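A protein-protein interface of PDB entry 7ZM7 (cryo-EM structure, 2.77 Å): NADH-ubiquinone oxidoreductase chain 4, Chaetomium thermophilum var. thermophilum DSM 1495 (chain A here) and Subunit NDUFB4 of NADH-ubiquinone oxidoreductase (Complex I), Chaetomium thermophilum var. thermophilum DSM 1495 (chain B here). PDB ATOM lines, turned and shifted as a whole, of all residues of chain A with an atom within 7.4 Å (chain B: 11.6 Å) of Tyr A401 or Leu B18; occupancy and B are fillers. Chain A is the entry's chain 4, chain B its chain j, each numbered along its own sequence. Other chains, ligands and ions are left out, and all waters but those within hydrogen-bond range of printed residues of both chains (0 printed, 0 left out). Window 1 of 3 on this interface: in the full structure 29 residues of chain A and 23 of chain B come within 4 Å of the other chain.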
ATOM      1  N   ARG A 335     -21.913  -8.716  16.623  1.00  0.00           N
ATOM      2  CA  ARG A 335     -21.562 -10.039  16.131  1.00  0.00           C
ATOM      3  C   ARG A 335     -22.741 -10.782  15.515  1.00  0.00           C
ATOM      4  O   ARG A 335     -22.705 -12.007  15.410  1.00  0.00           O
ATOM      5  CB  ARG A 335     -20.933 -10.853  17.257  1.00  0.00           C
ATOM      6  CG  ARG A 335     -19.621 -10.274  17.757  1.00  0.00           C
ATOM      7  CD  ARG A 335     -18.500 -10.332  16.740  1.00  0.00           C
ATOM      8  NE  ARG A 335     -18.145 -11.697  16.390  1.00  0.00           N
ATOM      9  CZ  ARG A 335     -17.377 -12.487  17.132  1.00  0.00           C
ATOM     10  NH1 ARG A 335     -16.892 -12.053  18.276  1.00  0.00           N
ATOM     11  NH2 ARG A 335     -17.109 -13.721  16.741  1.00  0.00           N
ATOM     12  N   THR A 336     -23.762 -10.068  15.070  1.00  0.00           N
ATOM     13  CA  THR A 336     -24.952 -10.688  14.507  1.00  0.00           C
ATOM     14  C   THR A 336     -24.817 -10.819  12.993  1.00  0.00           C
ATOM     15  O   THR A 336     -24.581  -9.829  12.298  1.00  0.00           O
ATOM     16  CB  THR A 336     -26.188  -9.866  14.871  1.00  0.00           C
ATOM     17  OG1 THR A 336     -26.136  -9.536  16.258  1.00  0.00           O
ATOM     18  CG2 THR A 336     -27.459 -10.656  14.618  1.00  0.00           C
ATOM     19  N   VAL A 337     -25.015 -12.030  12.480  1.00  0.00           N
ATOM     20  CA  VAL A 337     -24.802 -12.282  11.025  1.00  0.00           C
ATOM     21  C   VAL A 337     -26.133 -12.195  10.264  1.00  0.00           C
ATOM     22  O   VAL A 337     -26.087 -12.198   9.032  1.00  0.00           O
ATOM     23  CB  VAL A 337     -24.110 -13.647  10.818  1.00  0.00           C
ATOM     24  CG1 VAL A 337     -23.096 -13.928  11.908  1.00  0.00           C
ATOM     25  CG2 VAL A 337     -25.116 -14.787  10.753  1.00  0.00           C
ATOM     26  N   ASP A 338     -27.254 -12.070  10.975  1.00  0.00           N
ATOM     27  CA  ASP A 338     -28.583 -11.895  10.333  1.00  0.00           C
ATOM     28  C   ASP A 338     -28.888 -10.394  10.296  1.00  0.00           C
ATOM     29  O   ASP A 338     -28.845  -9.777  11.362  1.00  0.00           O
ATOM     30  CB  ASP A 338     -29.628 -12.716  11.089  1.00  0.00           C
ATOM     31  CG  ASP A 338     -30.979 -12.840  10.409  1.00  0.00           C
ATOM     32  OD1 ASP A 338     -31.601 -11.799  10.130  1.00  0.00           O
ATOM     33  OD2 ASP A 338     -31.405 -13.985  10.184  1.00  0.00           O
ATOM     34  N   VAL A 339     -29.150  -9.828   9.121  1.00  0.00           N
ATOM     35  CA  VAL A 339     -29.381  -8.359   8.987  1.00  0.00           C
ATOM     36  C   VAL A 339     -30.642  -7.942   9.751  1.00  0.00           C
ATOM     37  O   VAL A 339     -30.590  -6.929  10.465  1.00  0.00           O
ATOM     38  CB  VAL A 339     -29.484  -7.957   7.504  1.00  0.00           C
ATOM     39  CG1 VAL A 339     -29.646  -6.459   7.323  1.00  0.00           C
ATOM     40  CG2 VAL A 339     -28.292  -8.465   6.708  1.00  0.00           C
ATOM     41  N   THR A 397     -32.233 -14.210   1.291  1.00  0.00           N
ATOM     42  CA  THR A 397     -31.384 -14.550   2.458  1.00  0.00           C
ATOM     43  C   THR A 397     -31.207 -13.328   3.380  1.00  0.00           C
ATOM     44  O   THR A 397     -31.404 -12.205   2.898  1.00  0.00           O
ATOM     45  CB  THR A 397     -29.995 -15.047   2.026  1.00  0.00           C
ATOM     46  OG1 THR A 397     -29.286 -15.498   3.180  1.00  0.00           O
ATOM     47  CG2 THR A 397     -29.162 -14.010   1.305  1.00  0.00           C
ATOM     48  N   ARG A 398     -30.917 -13.545   4.671  1.00  0.00           N
ATOM     49  CA  ARG A 398     -30.606 -12.407   5.586  1.00  0.00           C
ATOM     50  C   ARG A 398     -29.162 -12.465   6.076  1.00  0.00           C
ATOM     51  O   ARG A 398     -28.830 -11.658   6.937  1.00  0.00           O
ATOM     52  CB  ARG A 398     -31.598 -12.269   6.743  1.00  0.00           C
ATOM     53  CG  ARG A 398     -32.824 -11.430   6.414  1.00  0.00           C
ATOM     54  CD  ARG A 398     -34.090 -12.145   6.831  1.00  0.00           C
ATOM     55  NE  ARG A 398     -35.310 -11.410   6.541  1.00  0.00           N
ATOM     56  CZ  ARG A 398     -36.531 -11.888   6.746  1.00  0.00           C
ATOM     57  NH1 ARG A 398     -36.689 -13.107   7.232  1.00  0.00           N
ATOM     58  NH2 ARG A 398     -37.589 -11.153   6.457  1.00  0.00           N
ATOM     59  N   LEU A 399     -28.358 -13.381   5.540  1.00  0.00           N
ATOM     60  CA  LEU A 399     -26.970 -13.532   6.041  1.00  0.00           C
ATOM     61  C   LEU A 399     -26.110 -12.411   5.467  1.00  0.00           C
ATOM     62  O   LEU A 399     -26.066 -12.294   4.242  1.00  0.00           O
ATOM     63  CB  LEU A 399     -26.444 -14.935   5.738  1.00  0.00           C
ATOM     64  CG  LEU A 399     -27.220 -16.086   6.369  1.00  0.00           C
ATOM     65  CD1 LEU A 399     -26.564 -17.415   6.038  1.00  0.00           C
ATOM     66  CD2 LEU A 399     -27.328 -15.903   7.873  1.00  0.00           C
ATOM     67  N   ILE A 400     -25.385 -11.676   6.314  1.00  0.00           N
ATOM     68  CA  ILE A 400     -24.630 -10.462   5.876  1.00  0.00           C
ATOM     69  C   ILE A 400     -23.381 -10.891   5.100  1.00  0.00           C
ATOM     70  O   ILE A 400     -22.673 -10.014   4.558  1.00  0.00           O
ATOM     71  CB  ILE A 400     -24.322  -9.547   7.083  1.00  0.00           C
ATOM     72  CG1 ILE A 400     -24.171  -8.079   6.683  1.00  0.00           C
ATOM     73  CG2 ILE A 400     -23.125 -10.051   7.876  1.00  0.00           C
ATOM     74  CD1 ILE A 400     -24.016  -7.145   7.855  1.00  0.00           C
ATOM     75  N   TYR A 401     -23.150 -12.199   5.001  1.00  0.00           N
ATOM     76  CA  TYR A 401     -21.964 -12.708   4.292  1.00  0.00           C
ATOM     77  C   TYR A 401     -22.207 -12.594   2.790  1.00  0.00           C
ATOM     78  O   TYR A 401     -21.221 -12.499   2.051  1.00  0.00           O
ATOM     79  CB  TYR A 401     -21.876 -14.210   4.547  1.00  0.00           C
ATOM     80  CG  TYR A 401     -21.768 -14.638   5.984  1.00  0.00           C
ATOM     81  CD1 TYR A 401     -20.644 -14.343   6.730  1.00  0.00           C
ATOM     82  CD2 TYR A 401     -22.770 -15.381   6.586  1.00  0.00           C
ATOM     83  CE1 TYR A 401     -20.526 -14.748   8.046  1.00  0.00           C
ATOM     84  CE2 TYR A 401     -22.669 -15.793   7.903  1.00  0.00           C
ATOM     85  CZ  TYR A 401     -21.543 -15.473   8.636  1.00  0.00           C
ATOM     86  OH  TYR A 401     -21.421 -15.874   9.934  1.00  0.00           O
ATOM     87  N   PHE A 402     -23.465 -12.564   2.348  1.00  0.00           N
ATOM     88  CA  PHE A 402     -23.713 -12.549   0.917  1.00  0.00           C
ATOM     89  C   PHE A 402     -23.794 -11.152   0.323  1.00  0.00           C
ATOM     90  O   PHE A 402     -23.929 -11.023  -0.895  1.00  0.00           O
ATOM     91  CB  PHE A 402     -25.005 -13.307   0.614  1.00  0.00           C
ATOM     92  CG  PHE A 402     -24.963 -14.747   1.003  1.00  0.00           C
ATOM     93  CD1 PHE A 402     -24.153 -15.636   0.326  1.00  0.00           C
ATOM     94  CD2 PHE A 402     -25.732 -15.217   2.050  1.00  0.00           C
ATOM     95  CE1 PHE A 402     -24.111 -16.956   0.675  1.00  0.00           C
ATOM     96  CE2 PHE A 402     -25.703 -16.536   2.402  1.00  0.00           C
ATOM     97  CZ  PHE A 402     -24.879 -17.412   1.720  1.00  0.00           C
ATOM     98  N   PHE A 403     -23.723 -10.109   1.135  1.00  0.00           N
ATOM     99  CA  PHE A 403     -23.935  -8.748   0.682  1.00  0.00           C
ATOM    100  C   PHE A 403     -22.613  -8.006   0.677  1.00  0.00           C
ATOM    101  O   PHE A 403     -21.730  -8.301   1.483  1.00  0.00           O
ATOM    102  CB  PHE A 403     -24.939  -8.032   1.571  1.00  0.00           C
ATOM    103  CG  PHE A 403     -26.289  -8.673   1.585  1.00  0.00           C
ATOM    104  CD1 PHE A 403     -27.202  -8.405   0.592  1.00  0.00           C
ATOM    105  CD2 PHE A 403     -26.649  -9.535   2.596  1.00  0.00           C
ATOM    106  CE1 PHE A 403     -28.422  -8.986   0.605  1.00  0.00           C
ATOM    107  CE2 PHE A 403     -27.874 -10.123   2.612  1.00  0.00           C
ATOM    108  CZ  PHE A 403     -28.762  -9.848   1.620  1.00  0.00           C
ATOM    109  N   ARG A 404     -22.468  -7.075  -0.258  1.00  0.00           N
ATOM    110  CA  ARG A 404     -21.268  -6.263  -0.353  1.00  0.00           C
ATOM    111  C   ARG A 404     -21.451  -5.246  -1.465  1.00  0.00           C
ATOM    112  O   ARG A 404     -21.924  -5.589  -2.548  1.00  0.00           O
ATOM    113  CB  ARG A 404     -20.042  -7.134  -0.634  1.00  0.00           C
ATOM    114  CG  ARG A 404     -18.736  -6.495  -0.288  1.00  0.00           C
ATOM    115  CD  ARG A 404     -17.574  -7.357  -0.700  1.00  0.00           C
ATOM    116  NE  ARG A 404     -17.724  -7.867  -2.058  1.00  0.00           N
ATOM    117  CZ  ARG A 404     -17.085  -8.928  -2.541  1.00  0.00           C
ATOM    118  NH1 ARG A 404     -16.237  -9.595  -1.789  1.00  0.00           N
ATOM    119  NH2 ARG A 404     -17.289  -9.315  -3.786  1.00  0.00           N
ATOM    120  N   ARG A 471     -20.631  -2.797   5.591  1.00  0.00           N
ATOM    121  CA  ARG A 471     -20.586  -4.180   5.076  1.00  0.00           C
ATOM    122  C   ARG A 471     -21.546  -4.380   3.898  1.00  0.00           C
ATOM    123  O   ARG A 471     -21.196  -5.147   2.995  1.00  0.00           O
ATOM    124  CB  ARG A 471     -20.828  -5.169   6.216  1.00  0.00           C
ATOM    125  CG  ARG A 471     -19.581  -5.514   7.017  1.00  0.00           C
ATOM    126  CD  ARG A 471     -19.941  -6.456   8.145  1.00  0.00           C
ATOM    127  NE  ARG A 471     -20.798  -5.815   9.128  1.00  0.00           N
ATOM    128  CZ  ARG A 471     -21.362  -6.443  10.150  1.00  0.00           C
ATOM    129  NH1 ARG A 471     -22.126  -5.777  10.997  1.00  0.00           N
ATOM    130  NH2 ARG A 471     -21.167  -7.737  10.316  1.00  0.00           N
ATOM    131  N   SER A 479     -21.121  -7.961  -4.663  1.00  0.00           N
ATOM    132  CA  SER A 479     -20.673  -9.267  -4.219  1.00  0.00           C
ATOM    133  C   SER A 479     -20.772 -10.289  -5.338  1.00  0.00           C
ATOM    134  O   SER A 479     -21.596 -10.182  -6.245  1.00  0.00           O
ATOM    135  CB  SER A 479     -21.493  -9.720  -3.015  1.00  0.00           C
ATOM    136  OG  SER A 479     -22.750 -10.219  -3.412  1.00  0.00           O
ATOM    137  N   TYR A 481     -21.628 -13.413  -4.963  1.00  0.00           N
ATOM    138  CA  TYR A 481     -22.740 -14.336  -4.814  1.00  0.00           C
ATOM    139  C   TYR A 481     -23.973 -13.868  -5.557  1.00  0.00           C
ATOM    140  O   TYR A 481     -24.905 -14.653  -5.732  1.00  0.00           O
ATOM    141  CB  TYR A 481     -23.065 -14.540  -3.338  1.00  0.00           C
ATOM    142  CG  TYR A 481     -21.854 -14.793  -2.488  1.00  0.00           C
ATOM    143  CD1 TYR A 481     -21.122 -13.745  -1.962  1.00  0.00           C
ATOM    144  CD2 TYR A 481     -21.443 -16.080  -2.201  1.00  0.00           C
ATOM    145  CE1 TYR A 481     -20.014 -13.973  -1.187  1.00  0.00           C
ATOM    146  CE2 TYR A 481     -20.327 -16.315  -1.425  1.00  0.00           C
ATOM    147  CZ  TYR A 481     -19.618 -15.259  -0.923  1.00  0.00           C
ATOM    148  OH  TYR A 481     -18.515 -15.483  -0.146  1.00  0.00           O
ATOM    149  N   ILE B   9     -28.963 -16.430  -6.688  1.00  0.00           N
ATOM    150  CA  ILE B   9     -27.853 -16.216  -5.709  1.00  0.00           C
ATOM    151  C   ILE B   9     -26.969 -17.456  -5.720  1.00  0.00           C
ATOM    152  O   ILE B   9     -27.529 -18.557  -5.685  1.00  0.00           O
ATOM    153  CB  ILE B   9     -28.407 -15.978  -4.291  1.00  0.00           C
ATOM    154  CG1 ILE B   9     -29.332 -14.764  -4.245  1.00  0.00           C
ATOM    155  CG2 ILE B   9     -27.269 -15.828  -3.294  1.00  0.00           C
ATOM    156  CD1 ILE B   9     -28.585 -13.460  -4.306  1.00  0.00           C
ATOM    157  N   ALA B  10     -25.657 -17.286  -5.837  1.00  0.00           N
ATOM    158  CA  ALA B  10     -24.738 -18.436  -5.729  1.00  0.00           C
ATOM    159  C   ALA B  10     -24.717 -18.839  -4.265  1.00  0.00           C
ATOM    160  O   ALA B  10     -23.738 -18.504  -3.586  1.00  0.00           O
ATOM    161  CB  ALA B  10     -23.357 -18.013  -6.136  1.00  0.00           C
ATOM    162  N   MET B  11     -25.778 -19.496  -3.801  1.00  0.00           N
ATOM    163  CA  MET B  11     -25.847 -19.821  -2.371  1.00  0.00           C
ATOM    164  C   MET B  11     -24.649 -20.709  -2.089  1.00  0.00           C
ATOM    165  O   MET B  11     -24.458 -21.700  -2.816  1.00  0.00           O
ATOM    166  CB  MET B  11     -27.154 -20.545  -2.074  1.00  0.00           C
ATOM    167  CG  MET B  11     -27.857 -20.017  -0.836  1.00  0.00           C
ATOM    168  SD  MET B  11     -27.995 -18.210  -0.808  1.00  0.00           S
ATOM    169  CE  MET B  11     -28.797 -17.958   0.774  1.00  0.00           C
ATOM    170  N   ASP B  12     -23.876 -20.349  -1.074  1.00  0.00           N
ATOM    171  CA  ASP B  12     -22.637 -21.088  -0.768  1.00  0.00           C
ATOM    172  C   ASP B  12     -22.973 -22.276   0.139  1.00  0.00           C
ATOM    173  O   ASP B  12     -23.461 -22.025   1.249  1.00  0.00           O
ATOM    174  CB  ASP B  12     -21.678 -20.158  -0.056  1.00  0.00           C
ATOM    175  CG  ASP B  12     -20.236 -20.476  -0.323  1.00  0.00           C
ATOM    176  OD1 ASP B  12     -19.828 -21.605  -0.007  1.00  0.00           O
ATOM    177  OD2 ASP B  12     -19.554 -19.583  -0.848  1.00  0.00           O
ATOM    178  N   PRO B  13     -22.713 -23.550  -0.235  1.00  0.00           N
ATOM    179  CA  PRO B  13     -22.970 -24.650   0.699  1.00  0.00           C
ATOM    180  C   PRO B  13     -22.289 -24.447   2.033  1.00  0.00           C
ATOM    181  O   PRO B  13     -22.821 -24.862   3.066  1.00  0.00           O
ATOM    182  CB  PRO B  13     -22.416 -25.874  -0.044  1.00  0.00           C
ATOM    183  CG  PRO B  13     -22.325 -25.457  -1.463  1.00  0.00           C
ATOM    184  CD  PRO B  13     -22.014 -24.008  -1.442  1.00  0.00           C
ATOM    185  N   ALA B  14     -21.129 -23.796   2.032  1.00  0.00           N
ATOM    186  CA  ALA B  14     -20.384 -23.584   3.262  1.00  0.00           C
ATOM    187  C   ALA B  14     -21.078 -22.575   4.155  1.00  0.00           C
ATOM    188  O   ALA B  14     -21.216 -22.788   5.362  1.00  0.00           O
ATOM    189  CB  ALA B  14     -18.968 -23.128   2.933  1.00  0.00           C
ATOM    190  N   LEU B  15     -21.511 -21.460   3.582  1.00  0.00           N
ATOM    191  CA  LEU B  15     -22.074 -20.385   4.385  1.00  0.00           C
ATOM    192  C   LEU B  15     -23.484 -20.715   4.852  1.00  0.00           C
ATOM    193  O   LEU B  15     -23.892 -20.304   5.942  1.00  0.00           O
ATOM    194  CB  LEU B  15     -22.042 -19.096   3.585  1.00  0.00           C
ATOM    195  CG  LEU B  15     -20.621 -18.642   3.292  1.00  0.00           C
ATOM    196  CD1 LEU B  15     -20.636 -17.515   2.305  1.00  0.00           C
ATOM    197  CD2 LEU B  15     -19.937 -18.204   4.570  1.00  0.00           C
ATOM    198  N   VAL B  16     -24.239 -21.461   4.049  1.00  0.00           N
ATOM    199  CA  VAL B  16     -25.575 -21.878   4.461  1.00  0.00           C
ATOM    200  C   VAL B  16     -25.504 -22.736   5.717  1.00  0.00           C
ATOM    201  O   VAL B  16     -26.261 -22.536   6.672  1.00  0.00           O
ATOM    202  CB  VAL B  16     -26.279 -22.609   3.306  1.00  0.00           C
ATOM    203  CG1 VAL B  16     -27.521 -23.294   3.769  1.00  0.00           C
ATOM    204  CG2 VAL B  16     -26.630 -21.629   2.233  1.00  0.00           C
ATOM    205  N   ARG B  17     -24.586 -23.692   5.746  1.00  0.00           N
ATOM    206  CA  ARG B  17     -24.474 -24.544   6.917  1.00  0.00           C
ATOM    207  C   ARG B  17     -23.886 -23.796   8.110  1.00  0.00           C
ATOM    208  O   ARG B  17     -24.132 -24.178   9.256  1.00  0.00           O
ATOM    209  CB  ARG B  17     -23.647 -25.778   6.572  1.00  0.00           C
ATOM    210  CG  ARG B  17     -22.198 -25.512   6.325  1.00  0.00           C
ATOM    211  CD  ARG B  17     -21.410 -26.800   6.322  1.00  0.00           C
ATOM    212  NE  ARG B  17     -21.273 -27.351   4.979  1.00  0.00           N
ATOM    213  CZ  ARG B  17     -20.214 -27.156   4.200  1.00  0.00           C
ATOM    214  NH1 ARG B  17     -20.175 -27.689   2.988  1.00  0.00           N
ATOM    215  NH2 ARG B  17     -19.190 -26.434   4.638  1.00  0.00           N
ATOM    216  N   LEU B  18     -23.106 -22.745   7.866  1.00  0.00           N
ATOM    217  CA  LEU B  18     -22.664 -21.886   8.956  1.00  0.00           C
ATOM    218  C   LEU B  18     -23.831 -21.152   9.598  1.00  0.00           C
ATOM    219  O   LEU B  18     -23.886 -21.015  10.824  1.00  0.00           O
ATOM    220  CB  LEU B  18     -21.638 -20.881   8.450  1.00  0.00           C
ATOM    221  CG  LEU B  18     -21.227 -19.805   9.452  1.00  0.00           C
ATOM    222  CD1 LEU B  18     -20.541 -20.410  10.647  1.00  0.00           C
ATOM    223  CD2 LEU B  18     -20.365 -18.778   8.792  1.00  0.00           C
ATOM    224  N   GLY B  19     -24.747 -20.632   8.788  1.00  0.00           N
ATOM    225  CA  GLY B  19     -25.945 -20.031   9.343  1.00  0.00           C
ATOM    226  C   GLY B  19     -26.849 -21.057   9.985  1.00  0.00           C
ATOM    227  O   GLY B  19     -27.406 -20.830  11.058  1.00  0.00           O
ATOM    228  N   SER B  20     -26.998 -22.209   9.344  1.00  0.00           N
ATOM    229  CA  SER B  20     -27.760 -23.285   9.952  1.00  0.00           C
ATOM    230  C   SER B  20     -27.105 -23.767  11.234  1.00  0.00           C
ATOM    231  O   SER B  20     -27.778 -24.342  12.097  1.00  0.00           O
ATOM    232  CB  SER B  20     -27.915 -24.424   8.959  1.00  0.00           C
ATOM    233  OG  SER B  20     -28.341 -23.910   7.716  1.00  0.00           O
ATOM    234  N   MET B  21     -25.801 -23.553  11.380  1.00  0.00           N
ATOM    235  CA  MET B  21     -25.164 -23.863  12.649  1.00  0.00           C
ATOM    236  C   MET B  21     -25.592 -22.882  13.729  1.00  0.00           C
ATOM    237  O   MET B  21     -25.883 -23.283  14.859  1.00  0.00           O
ATOM    238  CB  MET B  21     -23.650 -23.855  12.497  1.00  0.00           C
ATOM    239  CG  MET B  21     -22.930 -24.388  13.709  1.00  0.00           C
ATOM    240  SD  MET B  21     -22.486 -23.099  14.881  1.00  0.00           S
ATOM    241  CE  MET B  21     -20.996 -22.484  14.128  1.00  0.00           C
ATOM    242  N   ILE B  22     -25.627 -21.595  13.395  1.00  0.00           N
ATOM    243  CA  ILE B  22     -25.891 -20.554  14.379  1.00  0.00           C
ATOM    244  C   ILE B  22     -27.340 -20.603  14.844  1.00  0.00           C
ATOM    245  O   ILE B  22     -27.629 -20.503  16.040  1.00  0.00           O
ATOM    246  CB  ILE B  22     -25.525 -19.186  13.781  1.00  0.00           C
ATOM    247  CG1 ILE B  22     -24.033 -18.950  13.909  1.00  0.00           C
ATOM    248  CG2 ILE B  22     -26.245 -18.092  14.495  1.00  0.00           C
ATOM    249  CD1 ILE B  22     -23.513 -17.836  13.052  1.00  0.00           C
ATOM    250  N   SER B  23     -28.270 -20.781  13.910  1.00  0.00           N
ATOM    251  CA  SER B  23     -29.683 -20.794  14.255  1.00  0.00           C
ATOM    252  C   SER B  23     -30.034 -21.955  15.167  1.00  0.00           C
ATOM    253  O   SER B  23     -30.981 -21.859  15.955  1.00  0.00           O
ATOM    254  CB  SER B  23     -30.527 -20.850  12.988  1.00  0.00           C
ATOM    255  OG  SER B  23     -30.392 -19.653  12.249  1.00  0.00           O
ATOM    256  N   ASN B  24     -29.300 -23.057  15.068  1.00  0.00           N
ATOM    257  CA  ASN B  24     -29.543 -24.242  15.864  1.00  0.00           C
ATOM    258  C   ASN B  24     -28.555 -24.393  17.002  1.00  0.00           C
ATOM    259  O   ASN B  24     -28.533 -25.435  17.650  1.00  0.00           O
ATOM    260  CB  ASN B  24     -29.501 -25.473  14.972  1.00  0.00           C
ATOM    261  CG  ASN B  24     -30.700 -25.580  14.082  1.00  0.00           C
ATOM    262  OD1 ASN B  24     -31.753 -26.039  14.505  1.00  0.00           O
ATOM    263  ND2 ASN B  24     -30.555 -25.167  12.836  1.00  0.00           N
ATOM    264  N   ARG B  25     -27.754 -23.366  17.276  1.00  0.00           N
ATOM    265  CA  ARG B  25     -26.624 -23.492  18.195  1.00  0.00           C
ATOM    266  C   ARG B  25     -27.064 -23.855  19.609  1.00  0.00           C
ATOM    267  O   ARG B  25     -26.442 -24.698  20.254  1.00  0.00           O
ATOM    268  CB  ARG B  25     -25.841 -22.185  18.211  1.00  0.00           C
ATOM    269  CG  ARG B  25     -24.617 -22.223  19.061  1.00  0.00           C
ATOM    270  CD  ARG B  25     -23.839 -20.944  18.980  1.00  0.00           C
ATOM    271  NE  ARG B  25     -22.708 -20.989  19.894  1.00  0.00           N
ATOM    272  CZ  ARG B  25     -21.518 -21.489  19.604  1.00  0.00           C
ATOM    273  NH1 ARG B  25     -21.264 -21.959  18.399  1.00  0.00           N
ATOM    274  NH2 ARG B  25     -20.566 -21.490  20.514  1.00  0.00           N
ATOM    275  N   TYR B  26     -28.126 -23.227  20.101  1.00  0.00           N
ATOM    276  CA  TYR B  26     -28.542 -23.365  21.490  1.00  0.00           C
ATOM    277  C   TYR B  26     -28.941 -24.785  21.873  1.00  0.00           C
ATOM    278  O   TYR B  26     -28.978 -25.102  23.063  1.00  0.00           O
ATOM    279  CB  TYR B  26     -29.707 -22.412  21.755  1.00  0.00           C
ATOM    280  CG  TYR B  26     -30.970 -22.873  21.088  1.00  0.00           C
ATOM    281  CD1 TYR B  26     -31.167 -22.656  19.740  1.00  0.00           C
ATOM    282  CD2 TYR B  26     -31.936 -23.576  21.786  1.00  0.00           C
ATOM    283  CE1 TYR B  26     -32.278 -23.092  19.113  1.00  0.00           C
ATOM    284  CE2 TYR B  26     -33.058 -24.023  21.163  1.00  0.00           C
ATOM    285  CZ  TYR B  26     -33.224 -23.786  19.821  1.00  0.00           C
ATOM    286  OH  TYR B  26     -34.346 -24.225  19.172  1.00  0.00           O
ATOM    287  N   TYR B  28     -27.278 -27.288  21.718  1.00  0.00           N
ATOM    288  CA  TYR B  28     -26.102 -28.026  22.132  1.00  0.00           C
ATOM    289  C   TYR B  28     -25.360 -27.375  23.284  1.00  0.00           C
ATOM    290  O   TYR B  28     -24.292 -27.852  23.654  1.00  0.00           O
ATOM    291  CB  TYR B  28     -25.156 -28.234  20.953  1.00  0.00           C
ATOM    292  CG  TYR B  28     -25.824 -28.704  19.700  1.00  0.00           C
ATOM    293  CD1 TYR B  28     -26.540 -27.839  18.898  1.00  0.00           C
ATOM    294  CD2 TYR B  28     -25.808 -30.035  19.360  1.00  0.00           C
ATOM    295  CE1 TYR B  28     -27.152 -28.272  17.779  1.00  0.00           C
ATOM    296  CE2 TYR B  28     -26.427 -30.478  18.243  1.00  0.00           C
ATOM    297  CZ  TYR B  28     -27.097 -29.599  17.456  1.00  0.00           C
ATOM    298  OH  TYR B  28     -27.725 -30.057  16.324  1.00  0.00           O
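N of Ala B10 lies within hydrogen-bond range of O of Tyr A481, 2.7 Å away.
The backbone NH (N) of Ala B14 sits close to the side-chain carboxylate (OD1) of Asp B12, at 3.3 Å.
N of Leu A399 is in hydrogen-bond range of OG1 of Thr A397, at 3.3 Å.
The side-chain hydroxyl (OG) of Ser A479 is in hydrogen-bond range of the backbone carbonyl oxygen (O) of Phe A402, 2.9 Å away.
Met B11 touches Thr A397 (CE to CB, 3.4 Å).
O of Leu B15 touches CD1 of Leu A399 (3.9 Å).
Leu B18 touches Tyr A401 (CD2 to OH, 3.3 Å).
Phe A402 touches Met B11 (CE2 to CE, 3.8 Å).
CE1 of Phe A402 touches N of Asp B12 (3.8 Å).
Leu B15 touches Phe A402 (CB to CZ, 3.8 Å).
Tyr A481 touches Ile B9.
Asp B12 touches Tyr A481 (OD2 to CE2, 3.4 Å).
CD1 of Leu B15 touches OH of Tyr A481, at 3.8 Å.
No residue of chain B comes within 4 Å of Val A337.
Printed residues of chain B within 4 Å of Thr A397: Met B11.
Of chain B, only Leu B15 comes within 4 Å of Leu A399.
No residue of chain B comes within 4 Å of Ile A400.
Of chain B, only Leu B18 comes within 4 Å of Tyr A401.
Phe A402 touches just these residues of chain B: Met B11 (3.8 Å), Asp B12 (3.8 Å) and Leu B15 (3.8 Å).
Printed residues of chain B within 4 Å of Tyr A481: Ile B9 (3.3 Å), Ala B10 (2.7 Å), Asp B12 (3.4 Å) and Leu B15 (3.8 Å).
Of the printed residues of chain A, Ala B10 touches Tyr A481 (2.7 Å).
Of the printed residues of chain A, Leu B15 touches Leu A399, Phe A402 and Tyr A481.
Leu B18 touches just one residue of chain A: Tyr A401 (3.3 Å).
The nearest residue of chain A that does not touch Leu B18 is Leu A399 (5.8 Å).
Of the 16 printed residues of chain A, 5 touch a printed residue of chain B.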
